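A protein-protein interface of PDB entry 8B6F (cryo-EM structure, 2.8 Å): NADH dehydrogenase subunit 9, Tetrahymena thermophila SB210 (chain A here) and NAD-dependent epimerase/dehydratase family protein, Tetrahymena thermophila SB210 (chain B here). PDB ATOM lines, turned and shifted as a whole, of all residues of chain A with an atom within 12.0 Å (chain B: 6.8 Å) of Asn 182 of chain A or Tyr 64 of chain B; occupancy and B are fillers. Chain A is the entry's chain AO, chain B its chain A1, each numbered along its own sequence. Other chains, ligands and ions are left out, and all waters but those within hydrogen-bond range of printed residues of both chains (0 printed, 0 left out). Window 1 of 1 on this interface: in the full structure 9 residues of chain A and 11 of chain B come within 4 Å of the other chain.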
ATOM      1  N   ASP A 178     -19.123  -9.200 -17.646  1.00  0.00           N
ATOM      2  CA  ASP A 178     -17.995 -10.094 -17.426  1.00  0.00           C
ATOM      3  C   ASP A 178     -17.089  -9.527 -16.345  1.00  0.00           C
ATOM      4  O   ASP A 178     -16.942  -8.309 -16.210  1.00  0.00           O
ATOM      5  CB  ASP A 178     -17.179 -10.301 -18.708  1.00  0.00           C
ATOM      6  CG  ASP A 178     -17.886 -11.176 -19.718  1.00  0.00           C
ATOM      7  OD1 ASP A 178     -18.822 -11.903 -19.328  1.00  0.00           O
ATOM      8  OD2 ASP A 178     -17.499 -11.142 -20.904  1.00  0.00           O
ATOM      9  N   ALA A 179     -16.477 -10.425 -15.578  1.00  0.00           N
ATOM     10  CA  ALA A 179     -15.574 -10.053 -14.498  1.00  0.00           C
ATOM     11  C   ALA A 179     -14.133 -10.181 -14.974  1.00  0.00           C
ATOM     12  O   ALA A 179     -13.703 -11.264 -15.382  1.00  0.00           O
ATOM     13  CB  ALA A 179     -15.810 -10.927 -13.267  1.00  0.00           C
ATOM     14  N   PHE A 180     -13.397  -9.077 -14.921  1.00  0.00           N
ATOM     15  CA  PHE A 180     -11.983  -9.022 -15.264  1.00  0.00           C
ATOM     16  C   PHE A 180     -11.197  -8.529 -14.053  1.00  0.00           C
ATOM     17  O   PHE A 180     -11.748  -8.327 -12.969  1.00  0.00           O
ATOM     18  CB  PHE A 180     -11.748  -8.110 -16.472  1.00  0.00           C
ATOM     19  CG  PHE A 180     -12.372  -8.609 -17.741  1.00  0.00           C
ATOM     20  CD1 PHE A 180     -13.683  -8.295 -18.053  1.00  0.00           C
ATOM     21  CD2 PHE A 180     -11.641  -9.371 -18.635  1.00  0.00           C
ATOM     22  CE1 PHE A 180     -14.257  -8.746 -19.225  1.00  0.00           C
ATOM     23  CE2 PHE A 180     -12.210  -9.825 -19.808  1.00  0.00           C
ATOM     24  CZ  PHE A 180     -13.519  -9.508 -20.104  1.00  0.00           C
ATOM     25  N   TYR A 181      -9.898  -8.329 -14.245  1.00  0.00           N
ATOM     26  CA  TYR A 181      -9.035  -7.730 -13.237  1.00  0.00           C
ATOM     27  C   TYR A 181      -8.581  -6.357 -13.708  1.00  0.00           C
ATOM     28  O   TYR A 181      -8.074  -6.218 -14.825  1.00  0.00           O
ATOM     29  CB  TYR A 181      -7.822  -8.617 -12.961  1.00  0.00           C
ATOM     30  CG  TYR A 181      -6.780  -7.956 -12.093  1.00  0.00           C
ATOM     31  CD1 TYR A 181      -6.927  -7.905 -10.715  1.00  0.00           C
ATOM     32  CD2 TYR A 181      -5.650  -7.379 -12.653  1.00  0.00           C
ATOM     33  CE1 TYR A 181      -5.976  -7.299  -9.919  1.00  0.00           C
ATOM     34  CE2 TYR A 181      -4.693  -6.772 -11.867  1.00  0.00           C
ATOM     35  CZ  TYR A 181      -4.862  -6.735 -10.501  1.00  0.00           C
ATOM     36  OH  TYR A 181      -3.909  -6.130  -9.717  1.00  0.00           O
ATOM     37  N   ASN A 182      -8.761  -5.351 -12.856  1.00  0.00           N
ATOM     38  CA  ASN A 182      -8.369  -3.983 -13.166  1.00  0.00           C
ATOM     39  C   ASN A 182      -7.075  -3.659 -12.429  1.00  0.00           C
ATOM     40  O   ASN A 182      -7.012  -3.758 -11.199  1.00  0.00           O
ATOM     41  CB  ASN A 182      -9.479  -3.010 -12.779  1.00  0.00           C
ATOM     42  CG  ASN A 182      -9.294  -1.643 -13.400  1.00  0.00           C
ATOM     43  OD1 ASN A 182      -8.172  -1.216 -13.664  1.00  0.00           O
ATOM     44  ND2 ASN A 182     -10.399  -0.953 -13.644  1.00  0.00           N
ATOM     45  N   ILE A 183      -6.049  -3.267 -13.186  1.00  0.00           N
ATOM     46  CA  ILE A 183      -4.772  -2.873 -12.603  1.00  0.00           C
ATOM     47  C   ILE A 183      -4.897  -1.531 -11.901  1.00  0.00           C
ATOM     48  O   ILE A 183      -4.298  -1.311 -10.843  1.00  0.00           O
ATOM     49  CB  ILE A 183      -3.682  -2.859 -13.692  1.00  0.00           C
ATOM     50  CG1 ILE A 183      -3.382  -4.290 -14.148  1.00  0.00           C
ATOM     51  CG2 ILE A 183      -2.407  -2.202 -13.183  1.00  0.00           C
ATOM     52  CD1 ILE A 183      -2.620  -4.380 -15.450  1.00  0.00           C
ATOM     53  N   PHE A 184      -5.666  -0.607 -12.480  1.00  0.00           N
ATOM     54  CA  PHE A 184      -5.830   0.697 -11.853  1.00  0.00           C
ATOM     55  C   PHE A 184      -6.450   0.560 -10.470  1.00  0.00           C
ATOM     56  O   PHE A 184      -6.018   1.219  -9.518  1.00  0.00           O
ATOM     57  CB  PHE A 184      -6.683   1.602 -12.742  1.00  0.00           C
ATOM     58  CG  PHE A 184      -6.075   1.873 -14.089  1.00  0.00           C
ATOM     59  CD1 PHE A 184      -5.007   2.744 -14.219  1.00  0.00           C
ATOM     60  CD2 PHE A 184      -6.579   1.265 -15.227  1.00  0.00           C
ATOM     61  CE1 PHE A 184      -4.447   2.997 -15.455  1.00  0.00           C
ATOM     62  CE2 PHE A 184      -6.025   1.513 -16.468  1.00  0.00           C
ATOM     63  CZ  PHE A 184      -4.958   2.382 -16.581  1.00  0.00           C
ATOM     64  N   GLU A 185      -7.467  -0.290 -10.339  1.00  0.00           N
ATOM     65  CA  GLU A 185      -8.051  -0.601  -9.044  1.00  0.00           C
ATOM     66  C   GLU A 185      -7.369  -1.773  -8.351  1.00  0.00           C
ATOM     67  O   GLU A 185      -7.687  -2.055  -7.191  1.00  0.00           O
ATOM     68  CB  GLU A 185      -9.543  -0.900  -9.210  1.00  0.00           C
ATOM     69  CG  GLU A 185     -10.314   0.251  -9.834  1.00  0.00           C
ATOM     70  CD  GLU A 185     -11.788  -0.050  -9.998  1.00  0.00           C
ATOM     71  OE1 GLU A 185     -12.239  -1.102  -9.500  1.00  0.00           O
ATOM     72  OE2 GLU A 185     -12.497   0.766 -10.622  1.00  0.00           O
ATOM     73  N   ASN A 186      -6.446  -2.455  -9.027  1.00  0.00           N
ATOM     74  CA  ASN A 186      -5.669  -3.541  -8.431  1.00  0.00           C
ATOM     75  C   ASN A 186      -6.574  -4.607  -7.824  1.00  0.00           C
ATOM     76  O   ASN A 186      -6.304  -5.136  -6.744  1.00  0.00           O
ATOM     77  CB  ASN A 186      -4.698  -3.004  -7.380  1.00  0.00           C
ATOM     78  CG  ASN A 186      -3.571  -2.197  -7.985  1.00  0.00           C
ATOM     79  OD1 ASN A 186      -2.998  -2.576  -9.006  1.00  0.00           O
ATOM     80  ND2 ASN A 186      -3.246  -1.074  -7.357  1.00  0.00           N
ATOM     81  N   GLN A 187      -7.658  -4.934  -8.518  1.00  0.00           N
ATOM     82  CA  GLN A 187      -8.605  -5.903  -7.981  1.00  0.00           C
ATOM     83  C   GLN A 187      -9.574  -6.299  -9.087  1.00  0.00           C
ATOM     84  O   GLN A 187      -9.629  -5.671 -10.147  1.00  0.00           O
ATOM     85  CB  GLN A 187      -9.341  -5.332  -6.766  1.00  0.00           C
ATOM     86  CG  GLN A 187     -10.154  -6.345  -5.969  1.00  0.00           C
ATOM     87  CD  GLN A 187      -9.333  -7.552  -5.543  1.00  0.00           C
ATOM     88  OE1 GLN A 187      -9.810  -8.685  -5.585  1.00  0.00           O
ATOM     89  NE2 GLN A 187      -8.094  -7.312  -5.127  1.00  0.00           N
ATOM     90  N   VAL A 188     -10.342  -7.354  -8.818  1.00  0.00           N
ATOM     91  CA  VAL A 188     -11.335  -7.840  -9.768  1.00  0.00           C
ATOM     92  C   VAL A 188     -12.479  -6.841  -9.864  1.00  0.00           C
ATOM     93  O   VAL A 188     -13.005  -6.372  -8.847  1.00  0.00           O
ATOM     94  CB  VAL A 188     -11.839  -9.229  -9.352  1.00  0.00           C
ATOM     95  CG1 VAL A 188     -13.016  -9.668 -10.214  1.00  0.00           C
ATOM     96  CG2 VAL A 188     -10.716 -10.243  -9.443  1.00  0.00           C
ATOM     97  N   VAL A 189     -12.866  -6.508 -11.095  1.00  0.00           N
ATOM     98  CA  VAL A 189     -13.990  -5.626 -11.368  1.00  0.00           C
ATOM     99  C   VAL A 189     -14.921  -6.332 -12.347  1.00  0.00           C
ATOM    100  O   VAL A 189     -14.585  -7.365 -12.925  1.00  0.00           O
ATOM    101  CB  VAL A 189     -13.543  -4.260 -11.933  1.00  0.00           C
ATOM    102  CG1 VAL A 189     -12.449  -3.662 -11.074  1.00  0.00           C
ATOM    103  CG2 VAL A 189     -13.069  -4.393 -13.379  1.00  0.00           C
ATOM    104  N   VAL A 190     -16.105  -5.755 -12.526  1.00  0.00           N
ATOM    105  CA  VAL A 190     -17.106  -6.278 -13.447  1.00  0.00           C
ATOM    106  C   VAL A 190     -17.488  -5.163 -14.408  1.00  0.00           C
ATOM    107  O   VAL A 190     -17.730  -4.029 -13.985  1.00  0.00           O
ATOM    108  CB  VAL A 190     -18.343  -6.815 -12.701  1.00  0.00           C
ATOM    109  CG1 VAL A 190     -19.105  -5.688 -12.008  1.00  0.00           C
ATOM    110  CG2 VAL A 190     -19.246  -7.571 -13.651  1.00  0.00           C
ATOM    111  N   LEU A 191     -17.523  -5.479 -15.702  1.00  0.00           N
ATOM    112  CA  LEU A 191     -17.807  -4.493 -16.733  1.00  0.00           C
ATOM    113  C   LEU A 191     -18.691  -5.130 -17.798  1.00  0.00           C
ATOM    114  O   LEU A 191     -19.042  -6.312 -17.718  1.00  0.00           O
ATOM    115  CB  LEU A 191     -16.506  -3.932 -17.322  1.00  0.00           C
ATOM    116  CG  LEU A 191     -15.406  -4.922 -17.709  1.00  0.00           C
ATOM    117  CD1 LEU A 191     -15.784  -5.686 -18.964  1.00  0.00           C
ATOM    118  CD2 LEU A 191     -14.073  -4.221 -17.889  1.00  0.00           C
ATOM    119  N   LYS A 192     -19.054  -4.338 -18.804  1.00  0.00           N
ATOM    120  CA  LYS A 192     -19.986  -4.796 -19.822  1.00  0.00           C
ATOM    121  C   LYS A 192     -19.435  -6.028 -20.535  1.00  0.00           C
ATOM    122  O   LYS A 192     -18.241  -6.335 -20.476  1.00  0.00           O
ATOM    123  CB  LYS A 192     -20.269  -3.681 -20.827  1.00  0.00           C
ATOM    124  CG  LYS A 192     -21.593  -3.835 -21.556  1.00  0.00           C
ATOM    125  CD  LYS A 192     -21.978  -2.566 -22.301  1.00  0.00           C
ATOM    126  CE  LYS A 192     -21.040  -2.281 -23.463  1.00  0.00           C
ATOM    127  NZ  LYS A 192     -21.072  -3.361 -24.490  1.00  0.00           N
ATOM    128  N   ASN A 193     -20.325  -6.735 -21.224  1.00  0.00           N
ATOM    129  CA  ASN A 193     -20.047  -8.064 -21.748  1.00  0.00           C
ATOM    130  C   ASN A 193     -19.871  -8.023 -23.260  1.00  0.00           C
ATOM    131  O   ASN A 193     -20.718  -7.476 -23.974  1.00  0.00           O
ATOM    132  CB  ASN A 193     -21.179  -9.023 -21.374  1.00  0.00           C
ATOM    133  CG  ASN A 193     -20.903 -10.442 -21.798  1.00  0.00           C
ATOM    134  OD1 ASN A 193     -19.764 -10.806 -22.076  1.00  0.00           O
ATOM    135  ND2 ASN A 193     -21.947 -11.258 -21.844  1.00  0.00           N
ATOM    136  N   GLU A 194     -18.768  -8.597 -23.738  1.00  0.00           N
ATOM    137  CA  GLU A 194     -18.550  -8.865 -25.153  1.00  0.00           C
ATOM    138  C   GLU A 194     -18.088 -10.307 -25.292  1.00  0.00           C
ATOM    139  O   GLU A 194     -17.134 -10.719 -24.625  1.00  0.00           O
ATOM    140  CB  GLU A 194     -17.513  -7.916 -25.761  1.00  0.00           C
ATOM    141  CG  GLU A 194     -17.950  -6.461 -25.828  1.00  0.00           C
ATOM    142  CD  GLU A 194     -17.892  -5.765 -24.483  1.00  0.00           C
ATOM    143  OE1 GLU A 194     -17.472  -6.405 -23.497  1.00  0.00           O
ATOM    144  OE2 GLU A 194     -18.262  -4.573 -24.412  1.00  0.00           O
ATOM    145  N   GLY B  35     -14.965   0.824 -26.240  1.00  0.00           N
ATOM    146  CA  GLY B  35     -15.092  -0.609 -26.060  1.00  0.00           C
ATOM    147  C   GLY B  35     -14.268  -1.149 -24.911  1.00  0.00           C
ATOM    148  O   GLY B  35     -13.359  -0.478 -24.416  1.00  0.00           O
ATOM    149  N   ASN B  36     -14.586  -2.364 -24.474  1.00  0.00           N
ATOM    150  CA  ASN B  36     -13.873  -3.017 -23.387  1.00  0.00           C
ATOM    151  C   ASN B  36     -12.733  -3.861 -23.956  1.00  0.00           C
ATOM    152  O   ASN B  36     -12.379  -3.756 -25.133  1.00  0.00           O
ATOM    153  CB  ASN B  36     -14.846  -3.840 -22.546  1.00  0.00           C
ATOM    154  CG  ASN B  36     -15.767  -2.974 -21.709  1.00  0.00           C
ATOM    155  OD1 ASN B  36     -15.355  -1.943 -21.179  1.00  0.00           O
ATOM    156  ND2 ASN B  36     -17.020  -3.390 -21.589  1.00  0.00           N
ATOM    157  N   ARG B  37     -12.142  -4.713 -23.115  1.00  0.00           N
ATOM    158  CA  ARG B  37     -10.940  -5.443 -23.510  1.00  0.00           C
ATOM    159  C   ARG B  37     -11.154  -6.263 -24.775  1.00  0.00           C
ATOM    160  O   ARG B  37     -10.217  -6.440 -25.561  1.00  0.00           O
ATOM    161  CB  ARG B  37     -10.484  -6.353 -22.370  1.00  0.00           C
ATOM    162  CG  ARG B  37     -10.128  -5.608 -21.098  1.00  0.00           C
ATOM    163  CD  ARG B  37     -11.141  -5.858 -20.003  1.00  0.00           C
ATOM    164  NE  ARG B  37     -10.796  -5.155 -18.774  1.00  0.00           N
ATOM    165  CZ  ARG B  37      -9.876  -5.563 -17.910  1.00  0.00           C
ATOM    166  NH1 ARG B  37      -9.162  -6.655 -18.123  1.00  0.00           N
ATOM    167  NH2 ARG B  37      -9.667  -4.857 -16.803  1.00  0.00           N
ATOM    168  N   GLN B  38     -12.360  -6.776 -24.988  1.00  0.00           N
ATOM    169  CA  GLN B  38     -12.639  -7.638 -26.128  1.00  0.00           C
ATOM    170  C   GLN B  38     -12.993  -6.864 -27.391  1.00  0.00           C
ATOM    171  O   GLN B  38     -13.251  -7.486 -28.426  1.00  0.00           O
ATOM    172  CB  GLN B  38     -13.773  -8.608 -25.786  1.00  0.00           C
ATOM    173  CG  GLN B  38     -13.461  -9.529 -24.618  1.00  0.00           C
ATOM    174  CD  GLN B  38     -12.216 -10.363 -24.847  1.00  0.00           C
ATOM    175  OE1 GLN B  38     -11.812 -10.596 -25.985  1.00  0.00           O
ATOM    176  NE2 GLN B  38     -11.597 -10.811 -23.761  1.00  0.00           N
ATOM    177  N   SER B  39     -13.025  -5.537 -27.334  1.00  0.00           N
ATOM    178  CA  SER B  39     -13.289  -4.731 -28.514  1.00  0.00           C
ATOM    179  C   SER B  39     -12.008  -4.566 -29.331  1.00  0.00           C
ATOM    180  O   SER B  39     -10.935  -5.048 -28.961  1.00  0.00           O
ATOM    181  CB  SER B  39     -13.864  -3.377 -28.110  1.00  0.00           C
ATOM    182  OG  SER B  39     -14.166  -2.590 -29.249  1.00  0.00           O
ATOM    183  N   PRO B  56       3.374  -1.609 -16.552  1.00  0.00           N
ATOM    184  CA  PRO B  56       2.074  -2.305 -16.564  1.00  0.00           C
ATOM    185  C   PRO B  56       0.886  -1.364 -16.628  1.00  0.00           C
ATOM    186  O   PRO B  56      -0.099  -1.668 -17.312  1.00  0.00           O
ATOM    187  CB  PRO B  56       2.096  -3.119 -15.258  1.00  0.00           C
ATOM    188  CG  PRO B  56       3.176  -2.528 -14.434  1.00  0.00           C
ATOM    189  CD  PRO B  56       4.190  -2.008 -15.394  1.00  0.00           C
ATOM    190  N   GLY B  59       0.663   0.049 -20.217  1.00  0.00           N
ATOM    191  CA  GLY B  59       0.191  -0.995 -21.112  1.00  0.00           C
ATOM    192  C   GLY B  59      -1.285  -1.280 -20.931  1.00  0.00           C
ATOM    193  O   GLY B  59      -2.022  -1.447 -21.906  1.00  0.00           O
ATOM    194  N   ALA B  60      -1.738  -1.349 -19.680  1.00  0.00           N
ATOM    195  CA  ALA B  60      -3.147  -1.604 -19.416  1.00  0.00           C
ATOM    196  C   ALA B  60      -4.027  -0.474 -19.928  1.00  0.00           C
ATOM    197  O   ALA B  60      -5.163  -0.714 -20.350  1.00  0.00           O
ATOM    198  CB  ALA B  60      -3.364  -1.805 -17.920  1.00  0.00           C
ATOM    199  N   ALA B  61      -3.529   0.762 -19.892  1.00  0.00           N
ATOM    200  CA  ALA B  61      -4.306   1.889 -20.395  1.00  0.00           C
ATOM    201  C   ALA B  61      -4.764   1.641 -21.825  1.00  0.00           C
ATOM    202  O   ALA B  61      -5.935   1.844 -22.161  1.00  0.00           O
ATOM    203  CB  ALA B  61      -3.480   3.172 -20.308  1.00  0.00           C
ATOM    204  N   LEU B  62      -3.847   1.195 -22.685  1.00  0.00           N
ATOM    205  CA  LEU B  62      -4.204   0.897 -24.068  1.00  0.00           C
ATOM    206  C   LEU B  62      -4.932  -0.436 -24.188  1.00  0.00           C
ATOM    207  O   LEU B  62      -5.849  -0.572 -25.003  1.00  0.00           O
ATOM    208  CB  LEU B  62      -2.948   0.889 -24.939  1.00  0.00           C
ATOM    209  CG  LEU B  62      -2.120   2.175 -24.952  1.00  0.00           C
ATOM    210  CD1 LEU B  62      -0.903   2.010 -25.842  1.00  0.00           C
ATOM    211  CD2 LEU B  62      -2.955   3.357 -25.406  1.00  0.00           C
ATOM    212  N   GLY B  63      -4.536  -1.429 -23.393  1.00  0.00           N
ATOM    213  CA  GLY B  63      -5.107  -2.756 -23.546  1.00  0.00           C
ATOM    214  C   GLY B  63      -6.578  -2.819 -23.186  1.00  0.00           C
ATOM    215  O   GLY B  63      -7.352  -3.534 -23.828  1.00  0.00           O
ATOM    216  N   TYR B  64      -6.988  -2.079 -22.154  1.00  0.00           N
ATOM    217  CA  TYR B  64      -8.352  -2.193 -21.652  1.00  0.00           C
ATOM    218  C   TYR B  64      -9.398  -1.690 -22.633  1.00  0.00           C
ATOM    219  O   TYR B  64     -10.587  -1.958 -22.428  1.00  0.00           O
ATOM    220  CB  TYR B  64      -8.482  -1.438 -20.329  1.00  0.00           C
ATOM    221  CG  TYR B  64      -7.800  -2.144 -19.183  1.00  0.00           C
ATOM    222  CD1 TYR B  64      -7.144  -3.351 -19.383  1.00  0.00           C
ATOM    223  CD2 TYR B  64      -7.826  -1.617 -17.901  1.00  0.00           C
ATOM    224  CE1 TYR B  64      -6.530  -4.002 -18.363  1.00  0.00           C
ATOM    225  CE2 TYR B  64      -7.206  -2.272 -16.860  1.00  0.00           C
ATOM    226  CZ  TYR B  64      -6.561  -3.471 -17.109  1.00  0.00           C
ATOM    227  OH  TYR B  64      -5.925  -4.170 -16.124  1.00  0.00           O
ATOM    228  N   ILE B  65      -8.995  -0.976 -23.683  1.00  0.00           N
ATOM    229  CA  ILE B  65      -9.923  -0.548 -24.721  1.00  0.00           C
ATOM    230  C   ILE B  65      -9.869  -1.452 -25.942  1.00  0.00           C
ATOM    231  O   ILE B  65     -10.543  -1.171 -26.940  1.00  0.00           O
ATOM    232  CB  ILE B  65      -9.677   0.921 -25.117  1.00  0.00           C
ATOM    233  CG1 ILE B  65      -8.238   1.121 -25.596  1.00  0.00           C
ATOM    234  CG2 ILE B  65      -9.982   1.830 -23.935  1.00  0.00           C
ATOM    235  CD1 ILE B  65      -7.967   2.497 -26.159  1.00  0.00           C
ATOM    236  N   GLY B  66      -9.097  -2.534 -25.887  1.00  0.00           N
ATOM    237  CA  GLY B  66      -9.000  -3.476 -26.980  1.00  0.00           C
ATOM    238  C   GLY B  66      -7.771  -3.343 -27.850  1.00  0.00           C
ATOM    239  O   GLY B  66      -7.672  -4.049 -28.858  1.00  0.00           O
ATOM    240  N   SER B  67      -6.835  -2.468 -27.497  1.00  0.00           N
ATOM    241  CA  SER B  67      -5.652  -2.270 -28.316  1.00  0.00           C
ATOM    242  C   SER B  67      -4.706  -3.459 -28.204  1.00  0.00           C
ATOM    243  O   SER B  67      -4.656  -4.153 -27.187  1.00  0.00           O
ATOM    244  CB  SER B  67      -4.923  -0.996 -27.894  1.00  0.00           C
ATOM    245  OG  SER B  67      -5.804   0.113 -27.888  1.00  0.00           O
ATOM    246  N   VAL B  69      -1.030  -4.854 -27.737  1.00  0.00           N
ATOM    247  CA  VAL B  69       0.127  -4.369 -26.996  1.00  0.00           C
ATOM    248  C   VAL B  69       1.254  -5.381 -27.131  1.00  0.00           C
ATOM    249  O   VAL B  69       1.041  -6.584 -26.950  1.00  0.00           O
ATOM    250  CB  VAL B  69      -0.207  -4.115 -25.513  1.00  0.00           C
ATOM    251  CG1 VAL B  69      -1.231  -3.001 -25.384  1.00  0.00           C
ATOM    252  CG2 VAL B  69      -0.718  -5.381 -24.846  1.00  0.00           C
ATOM    253  N   LEU B  88      -1.606  -9.427 -18.393  1.00  0.00           N
ATOM    254  CA  LEU B  88      -2.954  -9.026 -18.014  1.00  0.00           C
ATOM    255  C   LEU B  88      -3.373  -7.693 -18.619  1.00  0.00           C
ATOM    256  O   LEU B  88      -4.531  -7.297 -18.454  1.00  0.00           O
ATOM    257  CB  LEU B  88      -3.066  -8.940 -16.489  1.00  0.00           C
ATOM    258  CG  LEU B  88      -2.852 -10.234 -15.704  1.00  0.00           C
ATOM    259  CD1 LEU B  88      -2.865  -9.960 -14.216  1.00  0.00           C
ATOM    260  CD2 LEU B  88      -3.910 -11.260 -16.059  1.00  0.00           C
ATOM    261  N   CYS B  89      -2.470  -6.994 -19.308  1.00  0.00           N
ATOM    262  CA  CYS B  89      -2.790  -5.658 -19.801  1.00  0.00           C
ATOM    263  C   CYS B  89      -3.928  -5.694 -20.813  1.00  0.00           C
ATOM    264  O   CYS B  89      -4.870  -4.899 -20.731  1.00  0.00           O
ATOM    265  CB  CYS B  89      -1.544  -5.020 -20.414  1.00  0.00           C
ATOM    266  SG  CYS B  89      -0.171  -4.835 -19.257  1.00  0.00           S
ATOM    267  N   ALA B  90      -3.863  -6.614 -21.778  1.00  0.00           N
ATOM    268  CA  ALA B  90      -4.857  -6.693 -22.842  1.00  0.00           C
ATOM    269  C   ALA B  90      -5.673  -7.976 -22.775  1.00  0.00           C
ATOM    270  O   ALA B  90      -6.904  -7.923 -22.709  1.00  0.00           O
ATOM    271  CB  ALA B  90      -4.172  -6.574 -24.210  1.00  0.00           C
ATOM    272  N   GLN B  94      -4.146 -10.434 -27.698  1.00  0.00           N
ATOM    273  CA  GLN B  94      -3.924  -9.000 -27.803  1.00  0.00           C
ATOM    274  C   GLN B  94      -2.627  -8.540 -27.159  1.00  0.00           C
ATOM    275  O   GLN B  94      -2.025  -7.584 -27.646  1.00  0.00           O
ATOM    276  CB  GLN B  94      -5.093  -8.235 -27.165  1.00  0.00           C
ATOM    277  CG  GLN B  94      -6.419  -8.447 -27.875  1.00  0.00           C
ATOM    278  CD  GLN B  94      -7.578  -7.809 -27.143  1.00  0.00           C
ATOM    279  OE1 GLN B  94      -7.558  -7.676 -25.921  1.00  0.00           O
ATOM    280  NE2 GLN B  94      -8.597  -7.400 -27.890  1.00  0.00           N
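The guanidinium group of Arg 37 of chain B lies within hydrogen-bond range of the backbone carbonyl oxygen of Tyr 181 of chain A (2.9 Å).
The backbone carbonyl oxygen of Lys 192 of chain A lies close to the side-chain amide nitrogen of Asn 36 of chain B (3.4 Å).
The side-chain hydroxyl (OH) of Tyr 64 of chain B lies within hydrogen-bond range of the backbone carbonyl oxygen (O) of Tyr 181 of chain A (3.2 Å).
The backbone NH of Ile 183 of chain A sits at hydrogen-bond distance from the side-chain hydroxyl of Tyr 64 of chain B, 3.1 Å away.
The side-chain amide nitrogen (ND2) of Asn 36 of chain B is in hydrogen-bond range of the side-chain carboxylate (OE2) of Glu 194 of chain A (3.3 Å).
The side-chain amide oxygen of Gln 94 of chain B sits close to the backbone carbonyl oxygen of Arg 37 of chain B, 3.0 Å away.
The backbone NH (N) of Asn 182 of chain A is in hydrogen-bond range of the backbone carbonyl oxygen (O) of Gln 187 of chain A, 2.9 Å away.
The backbone NH (N) of Arg 37 of chain B is in hydrogen-bond range of the backbone carbonyl oxygen (O) of Tyr 64 of chain B (3.2 Å).
The side-chain amide oxygen of Asn 182 of chain A lies within hydrogen-bond range of the backbone NH of Phe 184 of chain A (2.8 Å).
OD1 of Asn 186 of chain A lies close to O of Ile 183 of chain A, at 2.6 Å.
NZ of Lys 192 of chain A is in salt-bridge range of OE2 of Glu 194 of chain A, at 3.1 Å.
Among the printed residues, merely in contact across the chains: Phe 180 of chain A with Arg 37 of chain B (3.4 Å), Asn 182 of chain A with Tyr 64 of chain B (3.5 Å), Leu 191 of chain A with Arg 37 of chain B (3.5 Å), Ile 183 of chain A with Ala 60 of chain B (3.6 Å), Leu 191 of chain A with Asn 36 of chain B (3.7 Å), Glu 194 of chain A with Gln 38 of chain B (3.8 Å), Phe 184 of chain A with Tyr 64 of chain B (3.9 Å), Phe 184 of chain A with Ala 61 of chain B (3.9 Å) and Asn 182 of chain A with Arg 37 of chain B (3.96 Å).
Of chain B, only Arg 37 and Tyr 64 come within 4 Å of Asn 182 of chain A.
Of chain A, only Tyr 181 (3.2 Å), Asn 182 (3.5 Å), Ile 183 (3.1 Å) and Phe 184 (3.9 Å) come within 4 Å of Tyr 64 of chain B.
No residue of chain A comes within 4 Å of Gly 35 of chain B.
Asn 36 of chain B touches three residues of chain A.
Of chain A, only Phe 180 (3.4 Å), Tyr 181 (2.9 Å), Asn 182 (3.96 Å) and Leu 191 (3.5 Å) come within 4 Å of Arg 37 of chain B.
No residue of chain A comes within 4 Å of Ser 39 of chain B.
Of the printed residues of chain A, Ala 60 of chain B touches Ile 183.
Ala 61 of chain B touches just one residue of chain A: Phe 184 (3.9 Å).
No residue of chain A comes within 4 Å of Gly 66 of chain B.
No residue of chain A comes within 4 Å of Ser 67 of chain B.
No residue of chain A comes within 4 Å of Leu 88 of chain B.
No residue of chain A comes within 4 Å of Cys 89 of chain B.
No residue of chain A comes within 4 Å of Ala 90 of chain B.
Of the printed residues of chain B, Leu 191 of chain A touches Asn 36 and Arg 37.
Printed residues of chain B within 4 Å of Ile 183 of chain A: Ala 60 and Tyr 64.
Printed residues of chain B within 4 Å of Glu 194 of chain A: Asn 36 (3.3 Å) and Gln 38 (3.8 Å).
Of the printed residues of chain B, Phe 184 of chain A touches Ala 61 (3.9 Å) and Tyr 64 (3.9 Å).
Of the printed residues of chain B, Lys 192 of chain A touches Asn 36 (3.3 Å).
Val 190 of chain A touches none of the printed residues of chain B.
The nearest printed residue of chain B that does not touch Glu 194 of chain A is Ser 39 of chain B (5.2 Å).
Printed residues of chain B that touch a printed residue of chain A: Asn 36, Arg 37, Gln 38, Ala 60, Ala 61 and Tyr 64.
Among the printed residues, 14 pairs touch across the chains.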
